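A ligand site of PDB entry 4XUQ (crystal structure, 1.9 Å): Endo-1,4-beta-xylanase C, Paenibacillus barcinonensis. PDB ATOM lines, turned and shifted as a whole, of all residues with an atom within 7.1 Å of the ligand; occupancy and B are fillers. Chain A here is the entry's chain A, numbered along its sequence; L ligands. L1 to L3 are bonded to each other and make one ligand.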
ATOM      1  N   ARG A  31      16.953  30.245 -38.621  1.00  0.00           N
ATOM      2  CA  ARG A  31      17.710  29.796 -37.448  1.00  0.00           C
ATOM      3  C   ARG A  31      18.157  28.337 -37.556  1.00  0.00           C
ATOM      4  O   ARG A  31      18.980  27.855 -36.800  1.00  0.00           O
ATOM      5  CB  ARG A  31      16.865  29.998 -36.205  1.00  0.00           C
ATOM      6  CG  ARG A  31      16.333  31.406 -36.052  1.00  0.00           C
ATOM      7  CD  ARG A  31      15.707  31.624 -34.666  1.00  0.00           C
ATOM      8  NE  ARG A  31      16.688  31.719 -33.596  1.00  0.00           N
ATOM      9  CZ  ARG A  31      16.688  30.983 -32.481  1.00  0.00           C
ATOM     10  NH1 ARG A  31      15.723  30.118 -32.253  1.00  0.00           N
ATOM     11  NH2 ARG A  31      17.663  31.160 -31.572  1.00  0.00           N
ATOM     12  N   GLY A  32      17.553  27.585 -38.451  1.00  0.00           N
ATOM     13  CA  GLY A  32      17.987  26.218 -38.639  1.00  0.00           C
ATOM     14  C   GLY A  32      17.794  25.837 -40.069  1.00  0.00           C
ATOM     15  O   GLY A  32      18.292  26.496 -40.956  1.00  0.00           O
ATOM     16  N   THR A  58      10.231  24.159 -32.831  1.00  0.00           N
ATOM     17  CA  THR A  58       9.547  25.345 -32.330  1.00  0.00           C
ATOM     18  C   THR A  58      10.372  26.624 -32.517  1.00  0.00           C
ATOM     19  O   THR A  58       9.815  27.723 -32.686  1.00  0.00           O
ATOM     20  CB  THR A  58       9.200  25.268 -30.829  1.00  0.00           C
ATOM     21  OG1 THR A  58      10.388  25.110 -30.083  1.00  0.00           O
ATOM     22  CG2 THR A  58       8.251  24.092 -30.565  1.00  0.00           C
ATOM     23  N   TYR A  59      11.678  26.457 -32.465  1.00  0.00           N
ATOM     24  CA  TYR A  59      12.621  27.570 -32.481  1.00  0.00           C
ATOM     25  C   TYR A  59      13.006  28.054 -33.873  1.00  0.00           C
ATOM     26  O   TYR A  59      13.775  29.000 -34.028  1.00  0.00           O
ATOM     27  CB  TYR A  59      13.856  27.248 -31.619  1.00  0.00           C
ATOM     28  CG  TYR A  59      14.673  26.062 -32.081  1.00  0.00           C
ATOM     29  CD1 TYR A  59      15.537  26.184 -33.158  1.00  0.00           C
ATOM     30  CD2 TYR A  59      14.565  24.835 -31.426  1.00  0.00           C
ATOM     31  CE1 TYR A  59      16.297  25.107 -33.608  1.00  0.00           C
ATOM     32  CE2 TYR A  59      15.317  23.754 -31.854  1.00  0.00           C
ATOM     33  CZ  TYR A  59      16.192  23.917 -32.945  1.00  0.00           C
ATOM     34  OH  TYR A  59      16.941  22.874 -33.407  1.00  0.00           O
ATOM     35  N   HIS A  60      12.483  27.370 -34.884  1.00  0.00           N
ATOM     36  CA  HIS A  60      12.555  27.856 -36.232  1.00  0.00           C
ATOM     37  C   HIS A  60      11.642  29.053 -36.442  1.00  0.00           C
ATOM     38  O   HIS A  60      10.498  29.073 -36.000  1.00  0.00           O
ATOM     39  CB  HIS A  60      12.188  26.784 -37.243  1.00  0.00           C
ATOM     40  CG  HIS A  60      13.179  25.699 -37.346  1.00  0.00           C
ATOM     41  ND1 HIS A  60      12.903  24.517 -37.995  1.00  0.00           N
ATOM     42  CD2 HIS A  60      14.454  25.598 -36.938  1.00  0.00           C
ATOM     43  CE1 HIS A  60      13.963  23.739 -37.982  1.00  0.00           C
ATOM     44  NE2 HIS A  60      14.935  24.385 -37.377  1.00  0.00           N
ATOM     45  N   ASN A  94       5.722  33.858 -30.160  1.00  0.00           N
ATOM     46  CA  ASN A  94       6.608  34.582 -29.240  1.00  0.00           C
ATOM     47  C   ASN A  94       7.536  35.484 -30.019  1.00  0.00           C
ATOM     48  O   ASN A  94       8.009  35.089 -31.098  1.00  0.00           O
ATOM     49  CB  ASN A  94       7.476  33.606 -28.480  1.00  0.00           C
ATOM     50  CG  ASN A  94       6.706  32.757 -27.478  1.00  0.00           C
ATOM     51  OD1 ASN A  94       5.554  33.063 -27.096  1.00  0.00           O
ATOM     52  ND2 ASN A  94       7.345  31.708 -27.018  1.00  0.00           N
ATOM     53  N   SER A  96      11.287  36.902 -29.506  1.00  0.00           N
ATOM     54  CA  SER A  96      12.466  36.539 -28.709  1.00  0.00           C
ATOM     55  C   SER A  96      13.730  37.262 -29.190  1.00  0.00           C
ATOM     56  O   SER A  96      13.756  37.788 -30.295  1.00  0.00           O
ATOM     57  CB  SER A  96      12.690  35.035 -28.773  1.00  0.00           C
ATOM     58  OG  SER A  96      11.587  34.378 -28.155  1.00  0.00           O
ATOM     59  N   LEU A  97      14.718  37.271 -28.303  1.00  0.00           N
ATOM     60  CA  LEU A  97      16.039  37.820 -28.577  1.00  0.00           C
ATOM     61  C   LEU A  97      17.092  36.738 -28.482  1.00  0.00           C
ATOM     62  O   LEU A  97      17.026  35.918 -27.546  1.00  0.00           O
ATOM     63  CB  LEU A  97      16.356  38.902 -27.566  1.00  0.00           C
ATOM     64  CG  LEU A  97      15.386  40.047 -27.385  1.00  0.00           C
ATOM     65  CD1 LEU A  97      15.898  40.944 -26.293  1.00  0.00           C
ATOM     66  CD2 LEU A  97      15.213  40.788 -28.669  1.00  0.00           C
ATOM     67  N   GLU A  98      18.010  36.716 -29.436  1.00  0.00           N
ATOM     68  CA  GLU A  98      19.202  35.878 -29.401  1.00  0.00           C
ATOM     69  C   GLU A  98      20.381  36.794 -29.170  1.00  0.00           C
ATOM     70  O   GLU A  98      20.587  37.785 -29.912  1.00  0.00           O
ATOM     71  CB  GLU A  98      19.347  35.115 -30.691  1.00  0.00           C
ATOM     72  CG  GLU A  98      20.563  34.230 -30.811  1.00  0.00           C
ATOM     73  CD  GLU A  98      20.638  33.527 -32.139  1.00  0.00           C
ATOM     74  OE1 GLU A  98      19.786  32.686 -32.419  1.00  0.00           O
ATOM     75  OE2 GLU A  98      21.499  33.921 -32.992  1.00  0.00           O
ATOM     76  N   LEU A 108      25.488  31.180 -26.931  1.00  0.00           N
ATOM     77  CA  LEU A 108      24.407  32.136 -27.141  1.00  0.00           C
ATOM     78  C   LEU A 108      23.416  32.058 -26.016  1.00  0.00           C
ATOM     79  O   LEU A 108      23.299  31.013 -25.339  1.00  0.00           O
ATOM     80  CB  LEU A 108      23.670  31.836 -28.466  1.00  0.00           C
ATOM     81  CG  LEU A 108      24.550  31.951 -29.702  1.00  0.00           C
ATOM     82  CD1 LEU A 108      23.721  31.818 -30.951  1.00  0.00           C
ATOM     83  CD2 LEU A 108      25.249  33.296 -29.734  1.00  0.00           C
ATOM     84  N   GLU A 109      22.670  33.127 -25.811  1.00  0.00           N
ATOM     85  CA  GLU A 109      21.536  33.051 -24.938  1.00  0.00           C
ATOM     86  C   GLU A 109      20.288  33.565 -25.613  1.00  0.00           C
ATOM     87  O   GLU A 109      20.339  34.278 -26.615  1.00  0.00           O
ATOM     88  CB  GLU A 109      21.772  33.752 -23.595  1.00  0.00           C
ATOM     89  CG  GLU A 109      22.169  35.148 -23.633  1.00  0.00           C
ATOM     90  CD  GLU A 109      22.405  35.745 -22.265  1.00  0.00           C
ATOM     91  OE1 GLU A 109      21.571  36.519 -21.759  1.00  0.00           O
ATOM     92  OE2 GLU A 109      23.512  35.464 -21.712  1.00  0.00           O
ATOM     93  N   TYR A 110      19.166  33.198 -25.067  1.00  0.00           N
ATOM     94  CA  TYR A 110      17.861  33.509 -25.656  1.00  0.00           C
ATOM     95  C   TYR A 110      16.913  34.020 -24.594  1.00  0.00           C
ATOM     96  O   TYR A 110      16.890  33.494 -23.475  1.00  0.00           O
ATOM     97  CB  TYR A 110      17.302  32.251 -26.319  1.00  0.00           C
ATOM     98  CG  TYR A 110      18.327  31.485 -27.065  1.00  0.00           C
ATOM     99  CD1 TYR A 110      18.716  31.834 -28.334  1.00  0.00           C
ATOM    100  CD2 TYR A 110      18.945  30.391 -26.497  1.00  0.00           C
ATOM    101  CE1 TYR A 110      19.701  31.074 -29.010  1.00  0.00           C
ATOM    102  CE2 TYR A 110      19.911  29.661 -27.149  1.00  0.00           C
ATOM    103  CZ  TYR A 110      20.264  29.985 -28.391  1.00  0.00           C
ATOM    104  OH  TYR A 110      21.227  29.218 -29.051  1.00  0.00           O
ATOM    105  N   ALA A 111      16.073  34.982 -24.923  1.00  0.00           N
ATOM    106  CA  ALA A 111      15.033  35.472 -23.999  1.00  0.00           C
ATOM    107  C   ALA A 111      13.770  35.796 -24.765  1.00  0.00           C
ATOM    108  O   ALA A 111      13.850  36.394 -25.818  1.00  0.00           O
ATOM    109  CB  ALA A 111      15.498  36.672 -23.268  1.00  0.00           C
ATOM    110  N   MET A 112      12.621  35.393 -24.245  1.00  0.00           N
ATOM    111  CA  MET A 112      11.338  35.794 -24.827  1.00  0.00           C
ATOM    112  C   MET A 112      11.000  37.190 -24.351  1.00  0.00           C
ATOM    113  O   MET A 112      11.088  37.470 -23.181  1.00  0.00           O
ATOM    114  CB  MET A 112      10.254  34.860 -24.378  1.00  0.00           C
ATOM    115  CG  MET A 112       8.934  35.040 -25.127  1.00  0.00           C
ATOM    116  SD  MET A 112       7.593  34.317 -24.164  1.00  0.00           S
ATOM    117  CE  MET A 112       8.222  32.611 -23.984  1.00  0.00           C
ATOM    118  N   TYR A 145      13.786  37.676 -33.131  1.00  0.00           N
ATOM    119  CA  TYR A 145      13.168  36.617 -33.922  1.00  0.00           C
ATOM    120  C   TYR A 145      11.780  36.257 -33.389  1.00  0.00           C
ATOM    121  O   TYR A 145      11.418  36.645 -32.269  1.00  0.00           O
ATOM    122  CB  TYR A 145      14.064  35.370 -34.004  1.00  0.00           C
ATOM    123  CG  TYR A 145      14.297  34.586 -32.722  1.00  0.00           C
ATOM    124  CD1 TYR A 145      15.313  34.989 -31.839  1.00  0.00           C
ATOM    125  CD2 TYR A 145      13.634  33.403 -32.454  1.00  0.00           C
ATOM    126  CE1 TYR A 145      15.577  34.290 -30.680  1.00  0.00           C
ATOM    127  CE2 TYR A 145      13.917  32.652 -31.342  1.00  0.00           C
ATOM    128  CZ  TYR A 145      14.889  33.077 -30.445  1.00  0.00           C
ATOM    129  OH  TYR A 145      15.180  32.422 -29.280  1.00  0.00           O
ATOM    130  N   GLU A 147       9.046  32.911 -32.976  1.00  0.00           N
ATOM    131  CA  GLU A 147       9.008  31.468 -32.860  1.00  0.00           C
ATOM    132  C   GLU A 147       7.714  31.056 -32.149  1.00  0.00           C
ATOM    133  O   GLU A 147       6.940  31.898 -31.748  1.00  0.00           O
ATOM    134  CB  GLU A 147      10.213  30.969 -32.078  1.00  0.00           C
ATOM    135  CG  GLU A 147      10.221  31.465 -30.654  1.00  0.00           C
ATOM    136  CD  GLU A 147      11.357  30.960 -29.820  1.00  0.00           C
ATOM    137  OE1 GLU A 147      12.037  29.956 -30.186  1.00  0.00           O
ATOM    138  OE2 GLU A 147      11.607  31.609 -28.767  1.00  0.00           O
ATOM    139  N   THR A 148       7.518  29.765 -32.012  1.00  0.00           N
ATOM    140  CA  THR A 148       6.408  29.231 -31.217  1.00  0.00           C
ATOM    141  C   THR A 148       6.973  28.775 -29.889  1.00  0.00           C
ATOM    142  O   THR A 148       8.191  28.601 -29.762  1.00  0.00           O
ATOM    143  CB  THR A 148       5.633  28.091 -31.946  1.00  0.00           C
ATOM    144  OG1 THR A 148       6.543  27.149 -32.490  1.00  0.00           O
ATOM    145  CG2 THR A 148       4.839  28.686 -33.051  1.00  0.00           C
ATOM    146  N   PRO A 149       6.113  28.621 -28.857  1.00  0.00           N
ATOM    147  CA  PRO A 149       6.668  28.371 -27.499  1.00  0.00           C
ATOM    148  C   PRO A 149       7.581  27.173 -27.432  1.00  0.00           C
ATOM    149  O   PRO A 149       7.328  26.140 -28.057  1.00  0.00           O
ATOM    150  CB  PRO A 149       5.423  28.167 -26.645  1.00  0.00           C
ATOM    151  CG  PRO A 149       4.424  29.084 -27.289  1.00  0.00           C
ATOM    152  CD  PRO A 149       4.671  28.889 -28.765  1.00  0.00           C
ATOM    153  N   TRP A 150       8.695  27.390 -26.755  1.00  0.00           N
ATOM    154  CA  TRP A 150       9.742  26.453 -26.603  1.00  0.00           C
ATOM    155  C   TRP A 150       9.236  25.182 -26.010  1.00  0.00           C
ATOM    156  O   TRP A 150       8.489  25.176 -25.066  1.00  0.00           O
ATOM    157  CB  TRP A 150      10.832  27.025 -25.681  1.00  0.00           C
ATOM    158  CG  TRP A 150      11.836  26.046 -25.225  1.00  0.00           C
ATOM    159  CD1 TRP A 150      12.002  25.531 -23.931  1.00  0.00           C
ATOM    160  CD2 TRP A 150      12.834  25.445 -26.026  1.00  0.00           C
ATOM    161  NE1 TRP A 150      13.048  24.653 -23.921  1.00  0.00           N
ATOM    162  CE2 TRP A 150      13.583  24.586 -25.188  1.00  0.00           C
ATOM    163  CE3 TRP A 150      13.165  25.551 -27.345  1.00  0.00           C
ATOM    164  CZ2 TRP A 150      14.641  23.833 -25.674  1.00  0.00           C
ATOM    165  CZ3 TRP A 150      14.219  24.815 -27.830  1.00  0.00           C
ATOM    166  CH2 TRP A 150      14.951  23.977 -27.004  1.00  0.00           C
ATOM    167  N   LYS A 151       9.638  24.120 -26.682  1.00  0.00           N
ATOM    168  CA  LYS A 151       9.780  22.808 -26.093  1.00  0.00           C
ATOM    169  C   LYS A 151      10.652  21.972 -27.064  1.00  0.00           C
ATOM    170  O   LYS A 151      10.943  22.415 -28.201  1.00  0.00           O
ATOM    171  CB  LYS A 151       8.408  22.209 -25.764  1.00  0.00           C
ATOM    172  CG  LYS A 151       8.037  22.491 -24.310  1.00  0.00           C
ATOM    173  CD  LYS A 151       9.144  22.071 -23.370  1.00  0.00           C
ATOM    174  CE  LYS A 151       8.801  22.418 -21.946  1.00  0.00           C
ATOM    175  NZ  LYS A 151       9.928  21.998 -21.087  1.00  0.00           N
ATOM    176  N   GLN A 152      11.080  20.785 -26.623  1.00  0.00           N
ATOM    177  CA  GLN A 152      12.180  20.054 -27.307  1.00  0.00           C
ATOM    178  C   GLN A 152      11.752  19.195 -28.501  1.00  0.00           C
ATOM    179  O   GLN A 152      10.554  18.995 -28.710  1.00  0.00           O
ATOM    180  CB  GLN A 152      13.011  19.213 -26.323  1.00  0.00           C
ATOM    181  CG  GLN A 152      14.270  19.932 -25.818  1.00  0.00           C
ATOM    182  CD  GLN A 152      14.917  19.246 -24.631  1.00  0.00           C
ATOM    183  OE1 GLN A 152      14.532  18.148 -24.270  1.00  0.00           O
ATOM    184  NE2 GLN A 152      15.924  19.888 -23.995  1.00  0.00           N
HETATM  185  O1  LIG L   1      20.508  26.853 -32.546  1.00  0.00           O
HETATM  186  C1  LIG L   1      19.213  26.821 -31.928  1.00  0.00           C
HETATM  187  C2  LIG L   1      19.240  25.874 -30.717  1.00  0.00           C
HETATM  188  C3  LIG L   1      17.910  25.930 -29.963  1.00  0.00           C
HETATM  189  C4  LIG L   1      17.599  27.376 -29.631  1.00  0.00           C
HETATM  190  C5  LIG L   1      17.618  28.210 -30.846  1.00  0.00           C
HETATM  191  O2  LIG L   1      19.438  24.496 -31.102  1.00  0.00           O
HETATM  192  O3  LIG L   1      17.940  25.207 -28.744  1.00  0.00           O
HETATM  193  O4  LIG L   1      16.293  27.459 -29.129  1.00  0.00           O
HETATM  194  O5  LIG L   1      18.839  28.169 -31.506  1.00  0.00           O
HETATM  195  C1  LG2 L   2      16.072  28.493 -28.040  1.00  0.00           C
HETATM  196  C2  LG2 L   2      14.593  28.957 -28.143  1.00  0.00           C
HETATM  197  C3  LG2 L   2      14.313  29.892 -27.006  1.00  0.00           C
HETATM  198  C4  LG2 L   2      14.723  29.228 -25.672  1.00  0.00           C
HETATM  199  C5  LG2 L   2      16.150  28.660 -25.681  1.00  0.00           C
HETATM  200  O1  LG2 L   2      14.414  29.604 -29.394  1.00  0.00           O
HETATM  201  O2  LG2 L   2      12.907  30.221 -26.959  1.00  0.00           O
HETATM  202  O3  LG2 L   2      14.577  30.294 -24.721  1.00  0.00           O
HETATM  203  O4  LG2 L   2      16.285  27.775 -26.753  1.00  0.00           O
HETATM  204  C1  LG3 L   3      14.575  29.690 -23.207  1.00  0.00           C
HETATM  205  C2  LG3 L   3      14.929  30.936 -22.395  1.00  0.00           C
HETATM  206  C3  LG3 L   3      14.550  30.556 -20.987  1.00  0.00           C
HETATM  207  C4  LG3 L   3      13.098  30.071 -20.957  1.00  0.00           C
HETATM  208  C5  LG3 L   3      12.859  28.918 -21.924  1.00  0.00           C
HETATM  209  O1  LG3 L   3      16.339  31.224 -22.613  1.00  0.00           O
HETATM  210  O2  LG3 L   3      14.648  31.695 -20.144  1.00  0.00           O
HETATM  211  O3  LG3 L   3      12.868  29.609 -19.643  1.00  0.00           O
HETATM  212  O4  LG3 L   3      13.187  29.355 -23.231  1.00  0.00           O
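Merely in contact with the ligand: Tyr 59 (3.3 Å) and Trp 150 (3.6 Å). Hydrophobic or aromatic side chains within 4 Å of the ligand: Tyr 59, Tyr 110, Tyr 145 and Trp 150. Six residues have an atom within 4 Å of the ligand: Arg 31, Tyr 59, Tyr 110, Tyr 145, Glu 147 and Trp 150.
The side-chain carboxylate (OE2) of Glu 147 lies within hydrogen-bond range of the side-chain hydroxyl (OG) of Ser 96. The backbone NH (N) of Asn 94 sits at hydrogen-bond distance from the backbone carbonyl oxygen (O) of Glu 147. The backbone NH of Ser 96 is in hydrogen-bond range of the backbone carbonyl oxygen of Tyr 145 (2.8 Å). NH1 of Arg 31 sits at hydrogen-bond distance from O of Tyr 59, 2.9 Å away. NH2 of Arg 31 lies within salt-bridge range of OE1 of Glu 98, 2.7 Å away.
The backbone carbonyl oxygen (O) of Tyr 110 lies within hydrogen-bond range of an oxygen (O1) of LG3 L3, 2.5 Å away. The side-chain carboxylate (OE1) of Glu 147 sits at hydrogen-bond distance from an oxygen (O1) of LG2 L2. The side-chain hydroxyl (OH) of Tyr 145 sits at hydrogen-bond distance from an oxygen (O1) of LG2 L2, 2.9 Å away. O1 of LG2 L2 lies close to NH1 of Arg 31.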
